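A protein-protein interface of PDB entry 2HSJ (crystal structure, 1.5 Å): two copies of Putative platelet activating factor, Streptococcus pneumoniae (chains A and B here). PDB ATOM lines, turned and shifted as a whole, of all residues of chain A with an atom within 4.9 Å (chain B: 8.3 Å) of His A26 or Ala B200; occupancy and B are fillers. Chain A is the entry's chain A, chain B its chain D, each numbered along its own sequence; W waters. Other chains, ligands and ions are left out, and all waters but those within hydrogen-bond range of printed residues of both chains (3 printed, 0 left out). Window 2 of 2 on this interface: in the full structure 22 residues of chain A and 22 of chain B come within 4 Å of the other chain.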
ATOM      1  N   THR A  22      10.301  15.537   7.961  1.00  0.00           N
ATOM      2  CA  THR A  22       9.425  15.349   6.798  1.00  0.00           C
ATOM      3  C   THR A  22      10.176  14.583   5.707  1.00  0.00           C
ATOM      4  O   THR A  22       9.658  13.605   5.154  1.00  0.00           O
ATOM      5  CB  THR A  22       8.947  16.702   6.254  1.00  0.00           C
ATOM      6  OG1 THR A  22       8.125  17.321   7.263  1.00  0.00           O
ATOM      7  CG2 THR A  22       8.125  16.516   4.942  1.00  0.00           C
ATOM      8  N   LYS A  23      11.419  14.992   5.446  1.00  0.00           N
ATOM      9  CA  LYS A  23      12.223  14.355   4.404  1.00  0.00           C
ATOM     10  C   LYS A  23      12.409  12.869   4.695  1.00  0.00           C
ATOM     11  O   LYS A  23      12.202  12.009   3.815  1.00  0.00           O
ATOM     12  CB  LYS A  23      13.588  15.049   4.299  1.00  0.00           C
ATOM     13  CG  LYS A  23      14.521  14.536   3.228  1.00  0.00           C
ATOM     14  CD  LYS A  23      15.930  15.109   3.427  1.00  0.00           C
ATOM     15  CE  LYS A  23      16.798  14.773   2.208  1.00  0.00           C
ATOM     16  NZ  LYS A  23      18.205  15.319   2.399  1.00  0.00           N
ATOM     17  N   TYR A  24      12.796  12.558   5.935  1.00  0.00           N
ATOM     18  CA  TYR A  24      13.013  11.184   6.342  1.00  0.00           C
ATOM     19  C   TYR A  24      11.725  10.370   6.275  1.00  0.00           C
ATOM     20  O   TYR A  24      11.723   9.223   5.838  1.00  0.00           O
ATOM     21  CB  TYR A  24      13.551  11.154   7.769  1.00  0.00           C
ATOM     22  CG  TYR A  24      15.000  11.559   7.943  1.00  0.00           C
ATOM     23  CD1 TYR A  24      15.859  11.711   6.840  1.00  0.00           C
ATOM     24  CD2 TYR A  24      15.525  11.758   9.216  1.00  0.00           C
ATOM     25  CE1 TYR A  24      17.204  12.052   7.015  1.00  0.00           C
ATOM     26  CE2 TYR A  24      16.870  12.072   9.402  1.00  0.00           C
ATOM     27  CZ  TYR A  24      17.701  12.223   8.310  1.00  0.00           C
ATOM     28  OH  TYR A  24      19.035  12.547   8.478  1.00  0.00           O
ATOM     29  N   ARG A  25      10.631  10.943   6.753  1.00  0.00           N
ATOM     30  CA  ARG A  25       9.378  10.168   6.713  1.00  0.00           C
ATOM     31  C   ARG A  25       9.015   9.771   5.282  1.00  0.00           C
ATOM     32  O   ARG A  25       8.549   8.648   5.042  1.00  0.00           O
ATOM     33  CB  ARG A  25       8.195  10.904   7.376  1.00  0.00           C
ATOM     34  CG  ARG A  25       8.332  10.940   8.892  1.00  0.00           C
ATOM     35  CD  ARG A  25       7.134  11.599   9.573  1.00  0.00           C
ATOM     36  NE  ARG A  25       7.309  11.467  11.023  1.00  0.00           N
ATOM     37  CZ  ARG A  25       7.599  12.452  11.870  1.00  0.00           C
ATOM     38  NH1 ARG A  25       7.668  13.716  11.472  1.00  0.00           N
ATOM     39  NH2 ARG A  25       7.758  12.141  13.144  1.00  0.00           N
ATOM     40  N   HIS A  26       9.266  10.667   4.318  1.00  0.00           N
ATOM     41  CA  HIS A  26       8.945  10.337   2.927  1.00  0.00           C
ATOM     42  C   HIS A  26       9.967   9.339   2.367  1.00  0.00           C
ATOM     43  O   HIS A  26       9.588   8.360   1.701  1.00  0.00           O
ATOM     44  CB  HIS A  26       8.900  11.599   2.078  1.00  0.00           C
ATOM     45  CG  HIS A  26       8.213  11.419   0.756  1.00  0.00           C
ATOM     46  ND1 HIS A  26       7.608  12.471   0.100  1.00  0.00           N
ATOM     47  CD2 HIS A  26       8.007  10.325  -0.023  1.00  0.00           C
ATOM     48  CE1 HIS A  26       7.073  12.036  -1.031  1.00  0.00           C
ATOM     49  NE2 HIS A  26       7.310  10.742  -1.136  1.00  0.00           N
ATOM     50  N   LEU A  27      11.262   9.564   2.670  1.00  0.00           N
ATOM     51  CA  LEU A  27      12.276   8.579   2.239  1.00  0.00           C
ATOM     52  C   LEU A  27      12.019   7.171   2.751  1.00  0.00           C
ATOM     53  O   LEU A  27      12.252   6.184   2.044  1.00  0.00           O
ATOM     54  CB  LEU A  27      13.682   8.977   2.674  1.00  0.00           C
ATOM     55  CG  LEU A  27      14.306   9.977   1.729  1.00  0.00           C
ATOM     56  CD1 LEU A  27      15.610  10.514   2.359  1.00  0.00           C
ATOM     57  CD2 LEU A  27      14.554   9.392   0.304  1.00  0.00           C
ATOM     58  N   ASN A  28      11.561   7.076   3.993  1.00  0.00           N
ATOM     59  CA  ASN A  28      11.306   5.756   4.590  1.00  0.00           C
ATOM     60  C   ASN A  28      10.340   4.955   3.700  1.00  0.00           C
ATOM     61  O   ASN A  28      10.430   3.735   3.620  1.00  0.00           O
ATOM     62  CB  ASN A  28      10.703   5.886   5.984  1.00  0.00           C
ATOM     63  CG  ASN A  28      11.689   6.443   7.003  1.00  0.00           C
ATOM     64  OD1 ASN A  28      12.907   6.518   6.742  1.00  0.00           O
ATOM     65  ND2 ASN A  28      11.161   6.883   8.168  1.00  0.00           N
ATOM     66  N   HIS A  29       9.427   5.644   3.024  1.00  0.00           N
ATOM     67  CA  HIS A  29       8.431   4.967   2.179  1.00  0.00           C
ATOM     68  C   HIS A  29       8.964   4.634   0.789  1.00  0.00           C
ATOM     69  O   HIS A  29       8.632   3.577   0.218  1.00  0.00           O
ATOM     70  CB  HIS A  29       7.154   5.813   2.014  1.00  0.00           C
ATOM     71  CG  HIS A  29       6.391   6.040   3.285  1.00  0.00           C
ATOM     72  ND1 HIS A  29       5.804   5.018   3.991  1.00  0.00           N
ATOM     73  CD2 HIS A  29       6.103   7.180   3.959  1.00  0.00           C
ATOM     74  CE1 HIS A  29       5.226   5.509   5.075  1.00  0.00           C
ATOM     75  NE2 HIS A  29       5.375   6.821   5.068  1.00  0.00           N
ATOM     76  N   ILE A  30       9.779   5.515   0.218  1.00  0.00           N
ATOM     77  CA  ILE A  30      10.133   5.306  -1.192  1.00  0.00           C
ATOM     78  C   ILE A  30      11.581   4.886  -1.445  1.00  0.00           C
ATOM     79  O   ILE A  30      11.991   4.715  -2.600  1.00  0.00           O
ATOM     80  CB  ILE A  30       9.774   6.518  -2.060  1.00  0.00           C
ATOM     81  CG1 ILE A  30      10.654   7.720  -1.703  1.00  0.00           C
ATOM     82  CG2 ILE A  30       8.266   6.835  -1.932  1.00  0.00           C
ATOM     83  CD1 ILE A  30      10.793   8.722  -2.844  1.00  0.00           C
ATOM     84  N   PRO B  49      19.308  12.986  -1.675  1.00  0.00           N
ATOM     85  CA  PRO B  49      19.475  11.653  -1.049  1.00  0.00           C
ATOM     86  C   PRO B  49      19.862  10.637  -2.072  1.00  0.00           C
ATOM     87  O   PRO B  49      19.089   9.780  -2.490  1.00  0.00           O
ATOM     88  CB  PRO B  49      18.091  11.342  -0.452  1.00  0.00           C
ATOM     89  CG  PRO B  49      17.131  12.122  -1.326  1.00  0.00           C
ATOM     90  CD  PRO B  49      17.884  13.352  -1.858  1.00  0.00           C
ATOM     91  N   GLU B  52      19.645   6.662  -1.112  1.00  0.00           N
ATOM     92  CA  GLU B  52      18.319   6.084  -0.934  1.00  0.00           C
ATOM     93  C   GLU B  52      17.454   6.143  -2.190  1.00  0.00           C
ATOM     94  O   GLU B  52      16.446   5.421  -2.261  1.00  0.00           O
ATOM     95  CB  GLU B  52      17.633   6.700   0.285  1.00  0.00           C
ATOM     96  CG  GLU B  52      18.376   6.389   1.550  1.00  0.00           C
ATOM     97  CD  GLU B  52      17.624   6.904   2.755  1.00  0.00           C
ATOM     98  OE1 GLU B  52      16.683   6.238   3.222  1.00  0.00           O
ATOM     99  OE2 GLU B  52      17.952   8.020   3.221  1.00  0.00           O
ATOM    100  N   LEU B  53      17.841   6.980  -3.151  1.00  0.00           N
ATOM    101  CA  LEU B  53      17.043   7.045  -4.398  1.00  0.00           C
ATOM    102  C   LEU B  53      17.698   6.341  -5.581  1.00  0.00           C
ATOM    103  O   LEU B  53      16.982   5.904  -6.501  1.00  0.00           O
ATOM    104  CB  LEU B  53      16.675   8.496  -4.739  1.00  0.00           C
ATOM    105  CG  LEU B  53      15.800   9.174  -3.669  1.00  0.00           C
ATOM    106  CD1 LEU B  53      15.521  10.606  -4.124  1.00  0.00           C
ATOM    107  CD2 LEU B  53      14.474   8.455  -3.419  1.00  0.00           C
ATOM    108  N   CYS B 178      11.065  17.444 -17.195  1.00  0.00           N
ATOM    109  CA  CYS B 178      10.597  16.350 -16.325  1.00  0.00           C
ATOM    110  C   CYS B 178      10.031  16.814 -14.995  1.00  0.00           C
ATOM    111  O   CYS B 178       9.264  16.089 -14.361  1.00  0.00           O
ATOM    112  CB  CYS B 178      11.704  15.336 -16.050  1.00  0.00           C
ATOM    113  SG  CYS B 178      12.169  14.405 -17.548  1.00  0.00           S
ATOM    114  N   LEU B 179      10.424  18.010 -14.568  1.00  0.00           N
ATOM    115  CA  LEU B 179      10.045  18.513 -13.250  1.00  0.00           C
ATOM    116  C   LEU B 179       8.945  19.564 -13.330  1.00  0.00           C
ATOM    117  O   LEU B 179       8.449  20.010 -12.302  1.00  0.00           O
ATOM    118  CB  LEU B 179      11.262  19.068 -12.482  1.00  0.00           C
ATOM    119  CG  LEU B 179      12.370  18.054 -12.216  1.00  0.00           C
ATOM    120  CD1 LEU B 179      13.456  18.737 -11.400  1.00  0.00           C
ATOM    121  CD2 LEU B 179      11.826  16.812 -11.534  1.00  0.00           C
ATOM    122  N   LYS B 187       6.673  21.507 -10.419  1.00  0.00           N
ATOM    123  CA  LYS B 187       5.425  20.959  -9.848  1.00  0.00           C
ATOM    124  C   LYS B 187       5.340  21.222  -8.359  1.00  0.00           C
ATOM    125  O   LYS B 187       6.335  21.033  -7.632  1.00  0.00           O
ATOM    126  CB  LYS B 187       5.287  19.442 -10.101  1.00  0.00           C
ATOM    127  CG  LYS B 187       5.110  19.044 -11.555  1.00  0.00           C
ATOM    128  CD  LYS B 187       4.946  17.530 -11.785  1.00  0.00           C
ATOM    129  CE  LYS B 187       3.976  16.889 -10.799  1.00  0.00           C
ATOM    130  NZ  LYS B 187       3.592  15.460 -11.174  1.00  0.00           N
ATOM    131  N   LYS B 188       4.157  21.619  -7.893  1.00  0.00           N
ATOM    132  CA  LYS B 188       3.992  21.871  -6.471  1.00  0.00           C
ATOM    133  C   LYS B 188       4.457  20.670  -5.631  1.00  0.00           C
ATOM    134  O   LYS B 188       5.171  20.837  -4.631  1.00  0.00           O
ATOM    135  CB  LYS B 188       2.540  22.273  -6.141  1.00  0.00           C
ATOM    136  CG  LYS B 188       2.392  22.844  -4.734  1.00  0.00           C
ATOM    137  CD  LYS B 188       1.358  23.956  -4.673  1.00  0.00           C
ATOM    138  CE  LYS B 188       1.020  24.299  -3.246  1.00  0.00           C
ATOM    139  NZ  LYS B 188       0.089  23.270  -2.686  1.00  0.00           N
ATOM    140  N   GLU B 189       4.096  19.451  -6.044  1.00  0.00           N
ATOM    141  CA  GLU B 189       4.479  18.283  -5.259  1.00  0.00           C
ATOM    142  C   GLU B 189       5.979  18.037  -5.223  1.00  0.00           C
ATOM    143  O   GLU B 189       6.442  17.325  -4.353  1.00  0.00           O
ATOM    144  CB  GLU B 189       3.780  17.003  -5.704  1.00  0.00           C
ATOM    145  CG  GLU B 189       4.139  16.521  -7.052  1.00  0.00           C
ATOM    146  CD  GLU B 189       3.874  15.021  -7.238  1.00  0.00           C
ATOM    147  OE1 GLU B 189       4.242  14.202  -6.348  1.00  0.00           O
ATOM    148  OE2 GLU B 189       3.282  14.668  -8.282  1.00  0.00           O
ATOM    149  N   TYR B 190       6.711  18.623  -6.172  1.00  0.00           N
ATOM    150  CA  TYR B 190       8.147  18.375  -6.322  1.00  0.00           C
ATOM    151  C   TYR B 190       9.003  19.371  -5.551  1.00  0.00           C
ATOM    152  O   TYR B 190      10.225  19.251  -5.579  1.00  0.00           O
ATOM    153  CB  TYR B 190       8.528  18.406  -7.822  1.00  0.00           C
ATOM    154  CG  TYR B 190       8.048  17.246  -8.662  1.00  0.00           C
ATOM    155  CD1 TYR B 190       7.448  16.134  -8.090  1.00  0.00           C
ATOM    156  CD2 TYR B 190       8.193  17.283 -10.045  1.00  0.00           C
ATOM    157  CE1 TYR B 190       7.017  15.066  -8.877  1.00  0.00           C
ATOM    158  CE2 TYR B 190       7.790  16.244 -10.823  1.00  0.00           C
ATOM    159  CZ  TYR B 190       7.192  15.146 -10.243  1.00  0.00           C
ATOM    160  OH  TYR B 190       6.803  14.124 -11.092  1.00  0.00           O
ATOM    161  N   THR B 191       8.363  20.336  -4.894  1.00  0.00           N
ATOM    162  CA  THR B 191       9.098  21.420  -4.228  1.00  0.00           C
ATOM    163  C   THR B 191       8.741  21.597  -2.745  1.00  0.00           C
ATOM    164  O   THR B 191       7.610  21.315  -2.341  1.00  0.00           O
ATOM    165  CB  THR B 191       8.974  22.755  -5.000  1.00  0.00           C
ATOM    166  OG1 THR B 191       9.927  23.696  -4.498  1.00  0.00           O
ATOM    167  CG2 THR B 191       7.584  23.350  -4.870  1.00  0.00           C
ATOM    168  N   THR B 192       9.721  22.037  -1.957  1.00  0.00           N
ATOM    169  CA  THR B 192       9.456  22.448  -0.576  1.00  0.00           C
ATOM    170  C   THR B 192       9.142  23.936  -0.498  1.00  0.00           C
ATOM    171  O   THR B 192       8.164  24.316   0.135  1.00  0.00           O
ATOM    172  CB  THR B 192      10.640  22.136   0.352  1.00  0.00           C
ATOM    173  OG1 THR B 192      11.824  22.691  -0.212  1.00  0.00           O
ATOM    174  CG2 THR B 192      10.816  20.636   0.491  1.00  0.00           C
ATOM    175  N   LEU B 197      13.992  20.962  -3.802  1.00  0.00           N
ATOM    176  CA  LEU B 197      13.155  19.831  -4.138  1.00  0.00           C
ATOM    177  C   LEU B 197      12.642  19.110  -2.910  1.00  0.00           C
ATOM    178  O   LEU B 197      13.377  18.955  -1.915  1.00  0.00           O
ATOM    179  CB  LEU B 197      13.934  18.847  -5.008  1.00  0.00           C
ATOM    180  CG  LEU B 197      14.395  19.365  -6.369  1.00  0.00           C
ATOM    181  CD1 LEU B 197      14.997  18.219  -7.165  1.00  0.00           C
ATOM    182  CD2 LEU B 197      13.262  20.016  -7.214  1.00  0.00           C
ATOM    183  N   SER B 198      11.390  18.663  -2.984  1.00  0.00           N
ATOM    184  CA  SER B 198      10.857  17.700  -2.005  1.00  0.00           C
ATOM    185  C   SER B 198      11.385  16.300  -2.328  1.00  0.00           C
ATOM    186  O   SER B 198      12.005  16.073  -3.371  1.00  0.00           O
ATOM    187  CB  SER B 198       9.334  17.682  -2.126  1.00  0.00           C
ATOM    188  OG  SER B 198       9.000  17.152  -3.412  1.00  0.00           O
ATOM    189  N   ILE B 199      11.098  15.325  -1.472  1.00  0.00           N
ATOM    190  CA  ILE B 199      11.465  13.960  -1.795  1.00  0.00           C
ATOM    191  C   ILE B 199      10.797  13.457  -3.102  1.00  0.00           C
ATOM    192  O   ILE B 199      11.453  12.779  -3.914  1.00  0.00           O
ATOM    193  CB  ILE B 199      11.258  13.022  -0.572  1.00  0.00           C
ATOM    194  CG1 ILE B 199      12.289  13.338   0.529  1.00  0.00           C
ATOM    195  CG2 ILE B 199      11.321  11.562  -1.002  1.00  0.00           C
ATOM    196  CD1 ILE B 199      13.748  13.261   0.045  1.00  0.00           C
ATOM    197  N   ALA B 200       9.519  13.804  -3.310  1.00  0.00           N
ATOM    198  CA  ALA B 200       8.866  13.446  -4.595  1.00  0.00           C
ATOM    199  C   ALA B 200       9.615  14.077  -5.769  1.00  0.00           C
ATOM    200  O   ALA B 200       9.787  13.438  -6.807  1.00  0.00           O
ATOM    201  CB  ALA B 200       7.411  13.898  -4.618  1.00  0.00           C
ATOM    202  N   GLY B 201      10.065  15.320  -5.596  1.00  0.00           N
ATOM    203  CA  GLY B 201      10.878  15.999  -6.616  1.00  0.00           C
ATOM    204  C   GLY B 201      12.179  15.267  -6.896  1.00  0.00           C
ATOM    205  O   GLY B 201      12.532  15.010  -8.050  1.00  0.00           O
ATOM    206  N   TYR B 202      12.897  14.908  -5.832  1.00  0.00           N
ATOM    207  CA  TYR B 202      14.129  14.129  -6.021  1.00  0.00           C
ATOM    208  C   TYR B 202      13.867  12.758  -6.646  1.00  0.00           C
ATOM    209  O   TYR B 202      14.677  12.239  -7.431  1.00  0.00           O
ATOM    210  CB  TYR B 202      14.871  13.971  -4.689  1.00  0.00           C
ATOM    211  CG  TYR B 202      15.709  15.166  -4.291  1.00  0.00           C
ATOM    212  CD1 TYR B 202      16.856  15.499  -5.031  1.00  0.00           C
ATOM    213  CD2 TYR B 202      15.432  15.888  -3.128  1.00  0.00           C
ATOM    214  CE1 TYR B 202      17.662  16.568  -4.677  1.00  0.00           C
ATOM    215  CE2 TYR B 202      16.243  16.971  -2.748  1.00  0.00           C
ATOM    216  CZ  TYR B 202      17.367  17.283  -3.524  1.00  0.00           C
ATOM    217  OH  TYR B 202      18.167  18.334  -3.169  1.00  0.00           O
ATOM    218  N   GLN B 203      12.742  12.150  -6.313  1.00  0.00           N
ATOM    219  CA  GLN B 203      12.446  10.842  -6.902  1.00  0.00           C
ATOM    220  C   GLN B 203      12.262  11.014  -8.413  1.00  0.00           C
ATOM    221  O   GLN B 203      12.727  10.195  -9.218  1.00  0.00           O
ATOM    222  CB  GLN B 203      11.179  10.252  -6.261  1.00  0.00           C
ATOM    223  CG  GLN B 203      10.819   8.907  -6.857  1.00  0.00           C
ATOM    224  CD  GLN B 203       9.575   8.343  -6.241  1.00  0.00           C
ATOM    225  OE1 GLN B 203       8.555   9.037  -6.142  1.00  0.00           O
ATOM    226  NE2 GLN B 203       9.631   7.058  -5.854  1.00  0.00           N
ATOM    227  N   ALA B 204      11.546  12.080  -8.776  1.00  0.00           N
ATOM    228  CA  ALA B 204      11.266  12.338 -10.205  1.00  0.00           C
ATOM    229  C   ALA B 204      12.557  12.676 -10.947  1.00  0.00           C
ATOM    230  O   ALA B 204      12.777  12.204 -12.073  1.00  0.00           O
ATOM    231  CB  ALA B 204      10.275  13.482 -10.338  1.00  0.00           C
ATOM    232  N   LEU B 205      13.408  13.492 -10.323  1.00  0.00           N
ATOM    233  CA  LEU B 205      14.714  13.829 -10.900  1.00  0.00           C
ATOM    234  C   LEU B 205      15.552  12.573 -11.103  1.00  0.00           C
ATOM    235  O   LEU B 205      16.171  12.387 -12.148  1.00  0.00           O
ATOM    236  CB  LEU B 205      15.458  14.840 -10.001  1.00  0.00           C
ATOM    237  CG  LEU B 205      16.863  15.279 -10.472  1.00  0.00           C
ATOM    238  CD1 LEU B 205      16.854  15.834 -11.921  1.00  0.00           C
ATOM    239  CD2 LEU B 205      17.458  16.276  -9.489  1.00  0.00           C
ATOM    240  N   SER B 206      15.537  11.682 -10.111  1.00  0.00           N
ATOM    241  CA  SER B 206      16.310  10.458 -10.192  1.00  0.00           C
ATOM    242  C   SER B 206      15.846   9.547 -11.335  1.00  0.00           C
ATOM    243  O   SER B 206      16.664   8.938 -12.047  1.00  0.00           O
ATOM    244  CB  SER B 206      16.222   9.724  -8.854  1.00  0.00           C
ATOM    245  OG  SER B 206      16.767  10.520  -7.828  1.00  0.00           O
ATOM    246  N   LYS B 207      14.533   9.463 -11.518  1.00  0.00           N
ATOM    247  CA  LYS B 207      13.993   8.655 -12.606  1.00  0.00           C
ATOM    248  C   LYS B 207      14.456   9.229 -13.961  1.00  0.00           C
ATOM    249  O   LYS B 207      14.835   8.470 -14.860  1.00  0.00           O
ATOM    250  CB  LYS B 207      12.471   8.647 -12.522  1.00  0.00           C
ATOM    251  CG  LYS B 207      11.768   7.832 -13.593  1.00  0.00           C
ATOM    252  CD  LYS B 207      10.268   7.817 -13.284  1.00  0.00           C
ATOM    253  CE  LYS B 207       9.423   7.765 -14.544  1.00  0.00           C
ATOM    254  NZ  LYS B 207       9.064   6.383 -14.955  1.00  0.00           N
HETATM  255  O   HOH W   1      12.042   5.665  -5.223  1.00  0.00           O
HETATM  256  O   HOH W   2       6.360   9.953  -3.661  1.00  0.00           O
HETATM  257  O   HOH W   3       7.552  14.840  -1.352  1.00  0.00           O
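OG of Ser B198 sits close to N of Ala B200 (3.4 Å).
Water W3 lies within hydrogen-bond range of a ring nitrogen (ND1) of His A26, the backbone NH of Ala B200 and the side-chain hydroxyl of Ser B198.
Water W1 bridges the backbone carbonyl oxygen (O) of Ile A30 and the side-chain amide nitrogen (NE2) of Gln B203.
Water W2 bridges NE2 of His A26 (2.8 Å) and OE1 of Gln B203 (3.4 Å).
No position is printed for both chains.
Of the 10 pairs that touch across the chains among the printed residues, none has its exchanged pair printed and touching as well.
Among the printed residues, pairs that only touch across the chains: Ile A30 with Ile B199 (3.4 Å), Lys A23 with Ile B199 (3.5 Å), Leu A27 with Glu B52 (3.5 Å), His A26 with Ile B199 (3.6 Å), Ile A30 with Gln B203 (3.6 Å), Leu A27 with Ile B199 (3.7 Å), Ile A30 with Leu B53 (3.7 Å), His A26 with Ala B200 (3.8 Å), Leu A27 with Pro B49 (3.8 Å) and Leu A27 with Leu B53 (3.8 Å).
His A26 touches just these residues of chain B: Ile B199 (3.6 Å) and Ala B200 (3.8 Å).
Of chain A, only His A26 comes within 4 Å of Ala B200.
Of the printed residues of chain A, Pro B49 touches Leu A27 (3.8 Å).
Of the printed residues of chain A, Gln B203 touches Ile A30.
Of the printed residues of chain B, Ile A30 touches Leu B53 (3.7 Å), Ile B199 (3.4 Å) and Gln B203 (3.6 Å).
The nearest residue of chain B that does not touch His A26 is Gln B203 (5.4 Å).
The nearest printed residue of chain A that does not touch Ala B200 is Ile A30 (5.3 Å).
Of the 9 printed residues of chain A, 4 touch a printed residue of chain B.
Printed residues of chain A that touch a printed residue of chain B: Lys A23, His A26, Leu A27 and Ile A30.
Hydrophobic or aromatic side chains of chain A within 4 Å of the printed part of chain B: His A26, Leu A27 and Ile A30.
Among the printed residues, no Asp or Glu carboxylate lies within 4 Å of a Lys or Arg side-chain nitrogen of the other chain.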
